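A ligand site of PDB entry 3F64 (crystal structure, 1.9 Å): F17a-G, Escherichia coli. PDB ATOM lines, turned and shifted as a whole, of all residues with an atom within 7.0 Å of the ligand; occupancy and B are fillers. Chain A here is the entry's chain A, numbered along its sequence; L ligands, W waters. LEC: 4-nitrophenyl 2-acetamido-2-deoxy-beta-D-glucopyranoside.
The side-chain amide oxygen (OD1) of Asn 42 sits at hydrogen-bond distance from the backbone NH (N) of Asn 44 (2.8 Å).
The backbone carbonyl oxygen (O) of Trp 109 is in hydrogen-bond range of the backbone NH (N) of Val 54, 2.9 Å away.
The backbone carbonyl oxygen (O) of Gln 119 sits at hydrogen-bond distance from the backbone NH (N) of Val 45, at 2.9 Å.
The backbone NH (N) of Ser 117 lies within hydrogen-bond range of the backbone carbonyl oxygen (O) of Ile 48.
The backbone carbonyl oxygen (O) of Ala 43 lies within hydrogen-bond range of the side-chain hydroxyl (OG1) of Thr 118, at 3.1 Å.
OD1 of Asp 88 is in hydrogen-bond range of NE2 of Gln 119 (3.1 Å).
OG1 of Thr 89 lies within hydrogen-bond range of N of Leu 121 (3.4 Å).
OE1 of Gln 119 is in hydrogen-bond range of NE1 of Trp 109, at 2.8 Å.
An oxygen (O4) of the ligand lies within hydrogen-bond range of the side-chain amide nitrogen (NE2) of Gln 119, 3.2 Å away.
An oxygen (O3) of the ligand lies within hydrogen-bond range of the side-chain hydroxyl (OG1) of Thr 89, at 2.8 Å.
The backbone NH (N) of Gly 120 is in hydrogen-bond range of an oxygen (O4) of the ligand.
O of Ala 43 lies within hydrogen-bond range of O3 of the ligand.
OG1 of Thr 118 is in hydrogen-bond range of N2 of the ligand.
An oxygen (O4) of the ligand lies within hydrogen-bond range of the side-chain carboxylate (OD1) of Asp 88 (2.7 Å).
ND2 of Asn 44 lies within hydrogen-bond range of O7 of the ligand (3.4 Å).
O of Thr 118 sits close to N2 of the ligand, at 3.4 Å.
Trp 109 touches the ligand.
Ser 117 touches the ligand (OG to C1, 3.9 Å).
Hydrophobic or aromatic side chains that line the ligand: Ala 43 and Trp 109.
Nine residues have an atom within 4 Å of the ligand: Ala 43, Asn 44, Asp 88, Thr 89, Trp 109, Ser 117, Thr 118, Gln 119 and Gly 120.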
ATOM      1  N   ASN A  42      -0.112  17.796   8.376  1.00  0.00           N
ATOM      2  CA  ASN A  42       1.232  17.250   8.578  1.00  0.00           C
ATOM      3  C   ASN A  42       1.120  15.768   8.893  1.00  0.00           C
ATOM      4  O   ASN A  42       0.534  15.386   9.905  1.00  0.00           O
ATOM      5  CB  ASN A  42       1.919  17.992   9.730  1.00  0.00           C
ATOM      6  CG  ASN A  42       3.408  17.690   9.815  1.00  0.00           C
ATOM      7  OD1 ASN A  42       3.869  16.631   9.381  1.00  0.00           O
ATOM      8  ND2 ASN A  42       4.171  18.621  10.381  1.00  0.00           N
ATOM      9  N   ALA A  43       1.646  14.909   8.019  1.00  0.00           N
ATOM     10  CA  ALA A  43       1.597  13.482   8.266  1.00  0.00           C
ATOM     11  C   ALA A  43       2.550  13.010   9.388  1.00  0.00           C
ATOM     12  O   ALA A  43       2.444  11.875   9.847  1.00  0.00           O
ATOM     13  CB  ALA A  43       1.890  12.708   6.978  1.00  0.00           C
ATOM     14  N   ASN A  44       3.474  13.861   9.818  1.00  0.00           N
ATOM     15  CA  ASN A  44       4.560  13.412  10.712  1.00  0.00           C
ATOM     16  C   ASN A  44       4.713  14.301  11.952  1.00  0.00           C
ATOM     17  O   ASN A  44       5.598  15.157  12.000  1.00  0.00           O
ATOM     18  CB  ASN A  44       5.880  13.326   9.929  1.00  0.00           C
ATOM     19  CG  ASN A  44       5.722  12.595   8.593  1.00  0.00           C
ATOM     20  OD1 ASN A  44       5.778  13.201   7.503  1.00  0.00           O
ATOM     21  ND2 ASN A  44       5.506  11.290   8.658  1.00  0.00           N
ATOM     22  N   VAL A  45       3.834  14.104  12.940  1.00  0.00           N
ATOM     23  CA  VAL A  45       3.848  14.951  14.142  1.00  0.00           C
ATOM     24  C   VAL A  45       4.417  14.206  15.357  1.00  0.00           C
ATOM     25  O   VAL A  45       5.123  14.808  16.170  1.00  0.00           O
ATOM     26  CB  VAL A  45       2.443  15.573  14.436  1.00  0.00           C
ATOM     27  CG1 VAL A  45       2.468  16.486  15.662  1.00  0.00           C
ATOM     28  CG2 VAL A  45       1.938  16.352  13.218  1.00  0.00           C
ATOM     29  N   ILE A  48       6.156   6.980  16.169  1.00  0.00           N
ATOM     30  CA  ILE A  48       5.674   5.890  17.022  1.00  0.00           C
ATOM     31  C   ILE A  48       6.204   4.538  16.577  1.00  0.00           C
ATOM     32  O   ILE A  48       6.516   4.339  15.407  1.00  0.00           O
ATOM     33  CB  ILE A  48       4.124   5.855  17.132  1.00  0.00           C
ATOM     34  CG1 ILE A  48       3.468   5.591  15.763  1.00  0.00           C
ATOM     35  CG2 ILE A  48       3.593   7.138  17.724  1.00  0.00           C
ATOM     36  CD1 ILE A  48       1.972   5.241  15.870  1.00  0.00           C
ATOM     37  N   VAL A  54      -2.391   4.950  19.422  1.00  0.00           N
ATOM     38  CA  VAL A  54      -2.652   6.381  19.589  1.00  0.00           C
ATOM     39  C   VAL A  54      -3.799   6.943  18.706  1.00  0.00           C
ATOM     40  O   VAL A  54      -3.969   6.567  17.525  1.00  0.00           O
ATOM     41  CB  VAL A  54      -1.340   7.206  19.439  1.00  0.00           C
ATOM     42  CG1 VAL A  54      -0.815   7.139  17.996  1.00  0.00           C
ATOM     43  CG2 VAL A  54      -1.534   8.658  19.895  1.00  0.00           C
ATOM     44  N   LEU A  56      -6.359  10.964  18.537  1.00  0.00           N
ATOM     45  CA  LEU A  56      -6.239  12.415  18.712  1.00  0.00           C
ATOM     46  C   LEU A  56      -7.502  13.006  19.345  1.00  0.00           C
ATOM     47  O   LEU A  56      -8.622  12.580  19.025  1.00  0.00           O
ATOM     48  CB  LEU A  56      -6.022  13.140  17.357  1.00  0.00           C
ATOM     49  CG  LEU A  56      -4.854  12.760  16.436  1.00  0.00           C
ATOM     50  CD1 LEU A  56      -5.079  13.256  14.996  1.00  0.00           C
ATOM     51  CD2 LEU A  56      -3.511  13.272  16.987  1.00  0.00           C
ATOM     52  N   ASP A  88      -7.314  13.156  11.768  1.00  0.00           N
ATOM     53  CA  ASP A  88      -6.128  12.479  11.217  1.00  0.00           C
ATOM     54  C   ASP A  88      -5.611  13.229   9.989  1.00  0.00           C
ATOM     55  O   ASP A  88      -6.253  14.132   9.473  1.00  0.00           O
ATOM     56  CB  ASP A  88      -6.502  11.037  10.858  1.00  0.00           C
ATOM     57  CG  ASP A  88      -5.294  10.120  10.663  1.00  0.00           C
ATOM     58  OD1 ASP A  88      -4.195  10.432  11.186  1.00  0.00           O
ATOM     59  OD2 ASP A  88      -5.474   9.077   9.980  1.00  0.00           O
ATOM     60  N   THR A  89      -4.424  12.837   9.532  1.00  0.00           N
ATOM     61  CA  THR A  89      -3.724  13.526   8.459  1.00  0.00           C
ATOM     62  C   THR A  89      -4.568  13.866   7.227  1.00  0.00           C
ATOM     63  O   THR A  89      -4.588  15.019   6.790  1.00  0.00           O
ATOM     64  CB  THR A  89      -2.549  12.670   8.014  1.00  0.00           C
ATOM     65  OG1 THR A  89      -1.786  12.311   9.166  1.00  0.00           O
ATOM     66  CG2 THR A  89      -1.700  13.398   6.988  1.00  0.00           C
ATOM     67  N   LYS A  90      -5.238  12.875   6.655  1.00  0.00           N
ATOM     68  CA  LYS A  90      -5.986  13.102   5.406  1.00  0.00           C
ATOM     69  C   LYS A  90      -7.239  13.955   5.657  1.00  0.00           C
ATOM     70  O   LYS A  90      -7.987  13.689   6.597  1.00  0.00           O
ATOM     71  CB  LYS A  90      -6.336  11.775   4.713  1.00  0.00           C
ATOM     72  CG  LYS A  90      -5.150  11.007   4.139  1.00  0.00           C
ATOM     73  CD  LYS A  90      -5.631   9.832   3.290  1.00  0.00           C
ATOM     74  CE  LYS A  90      -4.530   8.801   3.006  1.00  0.00           C
ATOM     75  NZ  LYS A  90      -3.203   9.424   2.818  1.00  0.00           N
ATOM     76  N   ARG A  93     -10.840  12.708   6.453  1.00  0.00           N
ATOM     77  CA  ARG A  93     -11.058  12.144   7.816  1.00  0.00           C
ATOM     78  C   ARG A  93     -11.383  13.171   8.923  1.00  0.00           C
ATOM     79  O   ARG A  93     -11.526  12.798  10.095  1.00  0.00           O
ATOM     80  CB  ARG A  93      -9.844  11.325   8.245  1.00  0.00           C
ATOM     81  CG  ARG A  93      -9.285  10.409   7.176  1.00  0.00           C
ATOM     82  CD  ARG A  93      -9.573   8.968   7.459  1.00  0.00           C
ATOM     83  NE  ARG A  93      -8.359   8.214   7.201  1.00  0.00           N
ATOM     84  CZ  ARG A  93      -8.007   7.748   6.007  1.00  0.00           C
ATOM     85  NH1 ARG A  93      -8.792   7.938   4.943  1.00  0.00           N
ATOM     86  NH2 ARG A  93      -6.865   7.079   5.878  1.00  0.00           N
ATOM     87  N   PHE A 106     -10.102  11.547  16.235  1.00  0.00           N
ATOM     88  CA  PHE A 106      -9.564  10.380  15.532  1.00  0.00           C
ATOM     89  C   PHE A 106      -9.538   9.218  16.510  1.00  0.00           C
ATOM     90  O   PHE A 106      -8.813   9.240  17.514  1.00  0.00           O
ATOM     91  CB  PHE A 106      -8.154  10.661  14.959  1.00  0.00           C
ATOM     92  CG  PHE A 106      -7.472   9.440  14.337  1.00  0.00           C
ATOM     93  CD1 PHE A 106      -8.147   8.612  13.429  1.00  0.00           C
ATOM     94  CD2 PHE A 106      -6.138   9.151  14.634  1.00  0.00           C
ATOM     95  CE1 PHE A 106      -7.500   7.499  12.852  1.00  0.00           C
ATOM     96  CE2 PHE A 106      -5.496   8.051  14.057  1.00  0.00           C
ATOM     97  CZ  PHE A 106      -6.171   7.216  13.156  1.00  0.00           C
ATOM     98  N   GLY A 108      -8.212   6.337  16.325  1.00  0.00           N
ATOM     99  CA  GLY A 108      -6.836   5.867  16.542  1.00  0.00           C
ATOM    100  C   GLY A 108      -6.433   4.553  15.895  1.00  0.00           C
ATOM    101  O   GLY A 108      -7.265   3.831  15.309  1.00  0.00           O
ATOM    102  N   TRP A 109      -5.153   4.233  15.993  1.00  0.00           N
ATOM    103  CA  TRP A 109      -4.631   2.977  15.475  1.00  0.00           C
ATOM    104  C   TRP A 109      -3.410   2.545  16.264  1.00  0.00           C
ATOM    105  O   TRP A 109      -2.918   3.289  17.112  1.00  0.00           O
ATOM    106  CB  TRP A 109      -4.241   3.145  14.007  1.00  0.00           C
ATOM    107  CG  TRP A 109      -3.014   3.995  13.765  1.00  0.00           C
ATOM    108  CD1 TRP A 109      -2.837   5.317  14.087  1.00  0.00           C
ATOM    109  CD2 TRP A 109      -1.806   3.580  13.106  1.00  0.00           C
ATOM    110  NE1 TRP A 109      -1.590   5.746  13.678  1.00  0.00           N
ATOM    111  CE2 TRP A 109      -0.946   4.693  13.062  1.00  0.00           C
ATOM    112  CE3 TRP A 109      -1.381   2.375  12.540  1.00  0.00           C
ATOM    113  CZ2 TRP A 109       0.326   4.633  12.489  1.00  0.00           C
ATOM    114  CZ3 TRP A 109      -0.118   2.312  11.964  1.00  0.00           C
ATOM    115  CH2 TRP A 109       0.711   3.435  11.936  1.00  0.00           C
ATOM    116  N   CYS A 110      -2.920   1.353  15.963  1.00  0.00           N
ATOM    117  CA  CYS A 110      -1.737   0.798  16.630  1.00  0.00           C
ATOM    118  C   CYS A 110      -0.712   0.389  15.583  1.00  0.00           C
ATOM    119  O   CYS A 110      -1.016  -0.400  14.689  1.00  0.00           O
ATOM    120  CB  CYS A 110      -2.112  -0.432  17.467  1.00  0.00           C
ATOM    121  SG  CYS A 110      -3.393  -0.158  18.745  1.00  0.00           S
ATOM    122  N   VAL A 111       0.489   0.955  15.688  1.00  0.00           N
ATOM    123  CA  VAL A 111       1.630   0.565  14.876  1.00  0.00           C
ATOM    124  C   VAL A 111       2.037  -0.879  15.240  1.00  0.00           C
ATOM    125  O   VAL A 111       1.758  -1.364  16.347  1.00  0.00           O
ATOM    126  CB  VAL A 111       2.804   1.571  15.067  1.00  0.00           C
ATOM    127  CG1 VAL A 111       3.388   1.453  16.499  1.00  0.00           C
ATOM    128  CG2 VAL A 111       3.907   1.370  13.994  1.00  0.00           C
ATOM    129  N   GLY A 112       2.686  -1.566  14.310  1.00  0.00           N
ATOM    130  CA  GLY A 112       3.055  -2.957  14.531  1.00  0.00           C
ATOM    131  C   GLY A 112       4.042  -3.140  15.660  1.00  0.00           C
ATOM    132  O   GLY A 112       4.793  -2.215  16.003  1.00  0.00           O
ATOM    133  N   THR A 115       7.489  -2.497  14.082  1.00  0.00           N
ATOM    134  CA  THR A 115       7.685  -1.473  13.072  1.00  0.00           C
ATOM    135  C   THR A 115       7.637  -0.066  13.632  1.00  0.00           C
ATOM    136  O   THR A 115       7.267   0.154  14.776  1.00  0.00           O
ATOM    137  CB  THR A 115       6.726  -1.632  11.830  1.00  0.00           C
ATOM    138  OG1 THR A 115       5.399  -1.910  12.262  1.00  0.00           O
ATOM    139  CG2 THR A 115       7.184  -2.771  10.890  1.00  0.00           C
ATOM    140  N   ALA A 116       8.070   0.873  12.818  1.00  0.00           N
ATOM    141  CA  ALA A 116       8.046   2.265  13.156  1.00  0.00           C
ATOM    142  C   ALA A 116       7.195   2.979  12.111  1.00  0.00           C
ATOM    143  O   ALA A 116       7.186   2.616  10.934  1.00  0.00           O
ATOM    144  CB  ALA A 116       9.446   2.829  13.155  1.00  0.00           C
ATOM    145  N   SER A 117       6.480   4.002  12.545  1.00  0.00           N
ATOM    146  CA  SER A 117       5.721   4.838  11.629  1.00  0.00           C
ATOM    147  C   SER A 117       5.541   6.214  12.263  1.00  0.00           C
ATOM    148  O   SER A 117       6.299   6.570  13.176  1.00  0.00           O
ATOM    149  CB  SER A 117       4.372   4.194  11.290  1.00  0.00           C
ATOM    150  OG  SER A 117       3.692   4.918  10.258  1.00  0.00           O
ATOM    151  N   THR A 118       4.548   6.964  11.786  1.00  0.00           N
ATOM    152  CA  THR A 118       4.237   8.276  12.346  1.00  0.00           C
ATOM    153  C   THR A 118       2.717   8.476  12.522  1.00  0.00           C
ATOM    154  O   THR A 118       1.902   7.814  11.866  1.00  0.00           O
ATOM    155  CB  THR A 118       4.776   9.451  11.485  1.00  0.00           C
ATOM    156  OG1 THR A 118       4.219   9.374  10.166  1.00  0.00           O
ATOM    157  CG2 THR A 118       6.329   9.464  11.397  1.00  0.00           C
ATOM    158  N   GLN A 119       2.362   9.413  13.394  1.00  0.00           N
ATOM    159  CA  GLN A 119       0.977   9.882  13.569  1.00  0.00           C
ATOM    160  C   GLN A 119       0.933  11.346  13.157  1.00  0.00           C
ATOM    161  O   GLN A 119       1.792  12.131  13.557  1.00  0.00           O
ATOM    162  CB  GLN A 119       0.559   9.725  15.038  1.00  0.00           C
ATOM    163  CG  GLN A 119      -0.838  10.282  15.365  1.00  0.00           C
ATOM    164  CD  GLN A 119      -1.947   9.590  14.562  1.00  0.00           C
ATOM    165  OE1 GLN A 119      -2.032   8.368  14.521  1.00  0.00           O
ATOM    166  NE2 GLN A 119      -2.805  10.379  13.946  1.00  0.00           N
ATOM    167  N   GLY A 120      -0.023  11.719  12.309  1.00  0.00           N
ATOM    168  CA  GLY A 120      -0.102  13.083  11.813  1.00  0.00           C
ATOM    169  C   GLY A 120      -1.445  13.662  12.154  1.00  0.00           C
ATOM    170  O   GLY A 120      -2.173  13.114  13.000  1.00  0.00           O
ATOM    171  N   LEU A 121      -1.805  14.772  11.522  1.00  0.00           N
ATOM    172  CA  LEU A 121      -3.041  15.457  11.841  1.00  0.00           C
ATOM    173  C   LEU A 121      -3.420  16.457  10.763  1.00  0.00           C
ATOM    174  O   LEU A 121      -2.598  16.792   9.898  1.00  0.00           O
ATOM    175  CB  LEU A 121      -2.942  16.172  13.212  1.00  0.00           C
ATOM    176  CG  LEU A 121      -1.765  17.142  13.481  1.00  0.00           C
ATOM    177  CD1 LEU A 121      -1.910  18.431  12.698  1.00  0.00           C
ATOM    178  CD2 LEU A 121      -1.604  17.454  14.989  1.00  0.00           C
HETATM  179  C8  LEC L   1       2.087   8.500   6.086  1.00  0.00           C
HETATM  180  C7  LEC L   1       2.935   8.383   7.333  1.00  0.00           C
HETATM  181  O7  LEC L   1       4.191   8.496   7.277  1.00  0.00           O
HETATM  182  N2  LEC L   1       2.242   8.180   8.461  1.00  0.00           N
HETATM  183  C2  LEC L   1       0.772   8.062   8.531  1.00  0.00           C
HETATM  184  C3  LEC L   1       0.208   9.074   9.556  1.00  0.00           C
HETATM  185  O3  LEC L   1       0.285  10.412   9.022  1.00  0.00           O
HETATM  186  C4  LEC L   1      -1.250   8.750  10.004  1.00  0.00           C
HETATM  187  O4  LEC L   1      -1.626   9.603  11.112  1.00  0.00           O
HETATM  188  C5  LEC L   1      -1.405   7.265  10.396  1.00  0.00           C
HETATM  189  C6  LEC L   1      -2.863   6.910  10.811  1.00  0.00           C
HETATM  190  O6  LEC L   1      -3.738   6.978   9.691  1.00  0.00           O
HETATM  191  O5  LEC L   1      -0.970   6.383   9.322  1.00  0.00           O
HETATM  192  C1  LEC L   1       0.419   6.595   8.883  1.00  0.00           C
HETATM  193  O1  LEC L   1       0.623   5.830   7.662  1.00  0.00           O
HETATM  194  C1' LEC L   1       0.641   4.453   7.718  1.00  0.00           C
HETATM  195  C2' LEC L   1      -0.325   3.729   8.401  1.00  0.00           C
HETATM  196  C3' LEC L   1      -0.308   2.328   8.418  1.00  0.00           C
HETATM  197  C4' LEC L   1       0.688   1.634   7.733  1.00  0.00           C
HETATM  198  N1' LEC L   1       0.743   0.295   7.721  1.00  0.00           N
HETATM  199  O2' LEC L   1      -0.093  -0.513   8.501  1.00  0.00           O
HETATM  200  O1' LEC L   1       1.709  -0.336   6.932  1.00  0.00           O
HETATM  201  C5' LEC L   1       1.649   2.372   7.050  1.00  0.00           C
HETATM  202  C6' LEC L   1       1.629   3.756   7.030  1.00  0.00           C
HETATM  203  O   HOH W   1      -0.721  10.115   5.812  1.00  0.00           O
HETATM  204  O   HOH W   2       3.238   9.889   3.932  1.00  0.00           O
HETATM  205  O   HOH W   3      -0.916  -0.980   5.012  1.00  0.00           O
HETATM  206  O   HOH W   4      -2.451   0.385   6.814  1.00  0.00           O
HETATM  207  O   HOH W   5       4.024   0.106   9.298  1.00  0.00           O
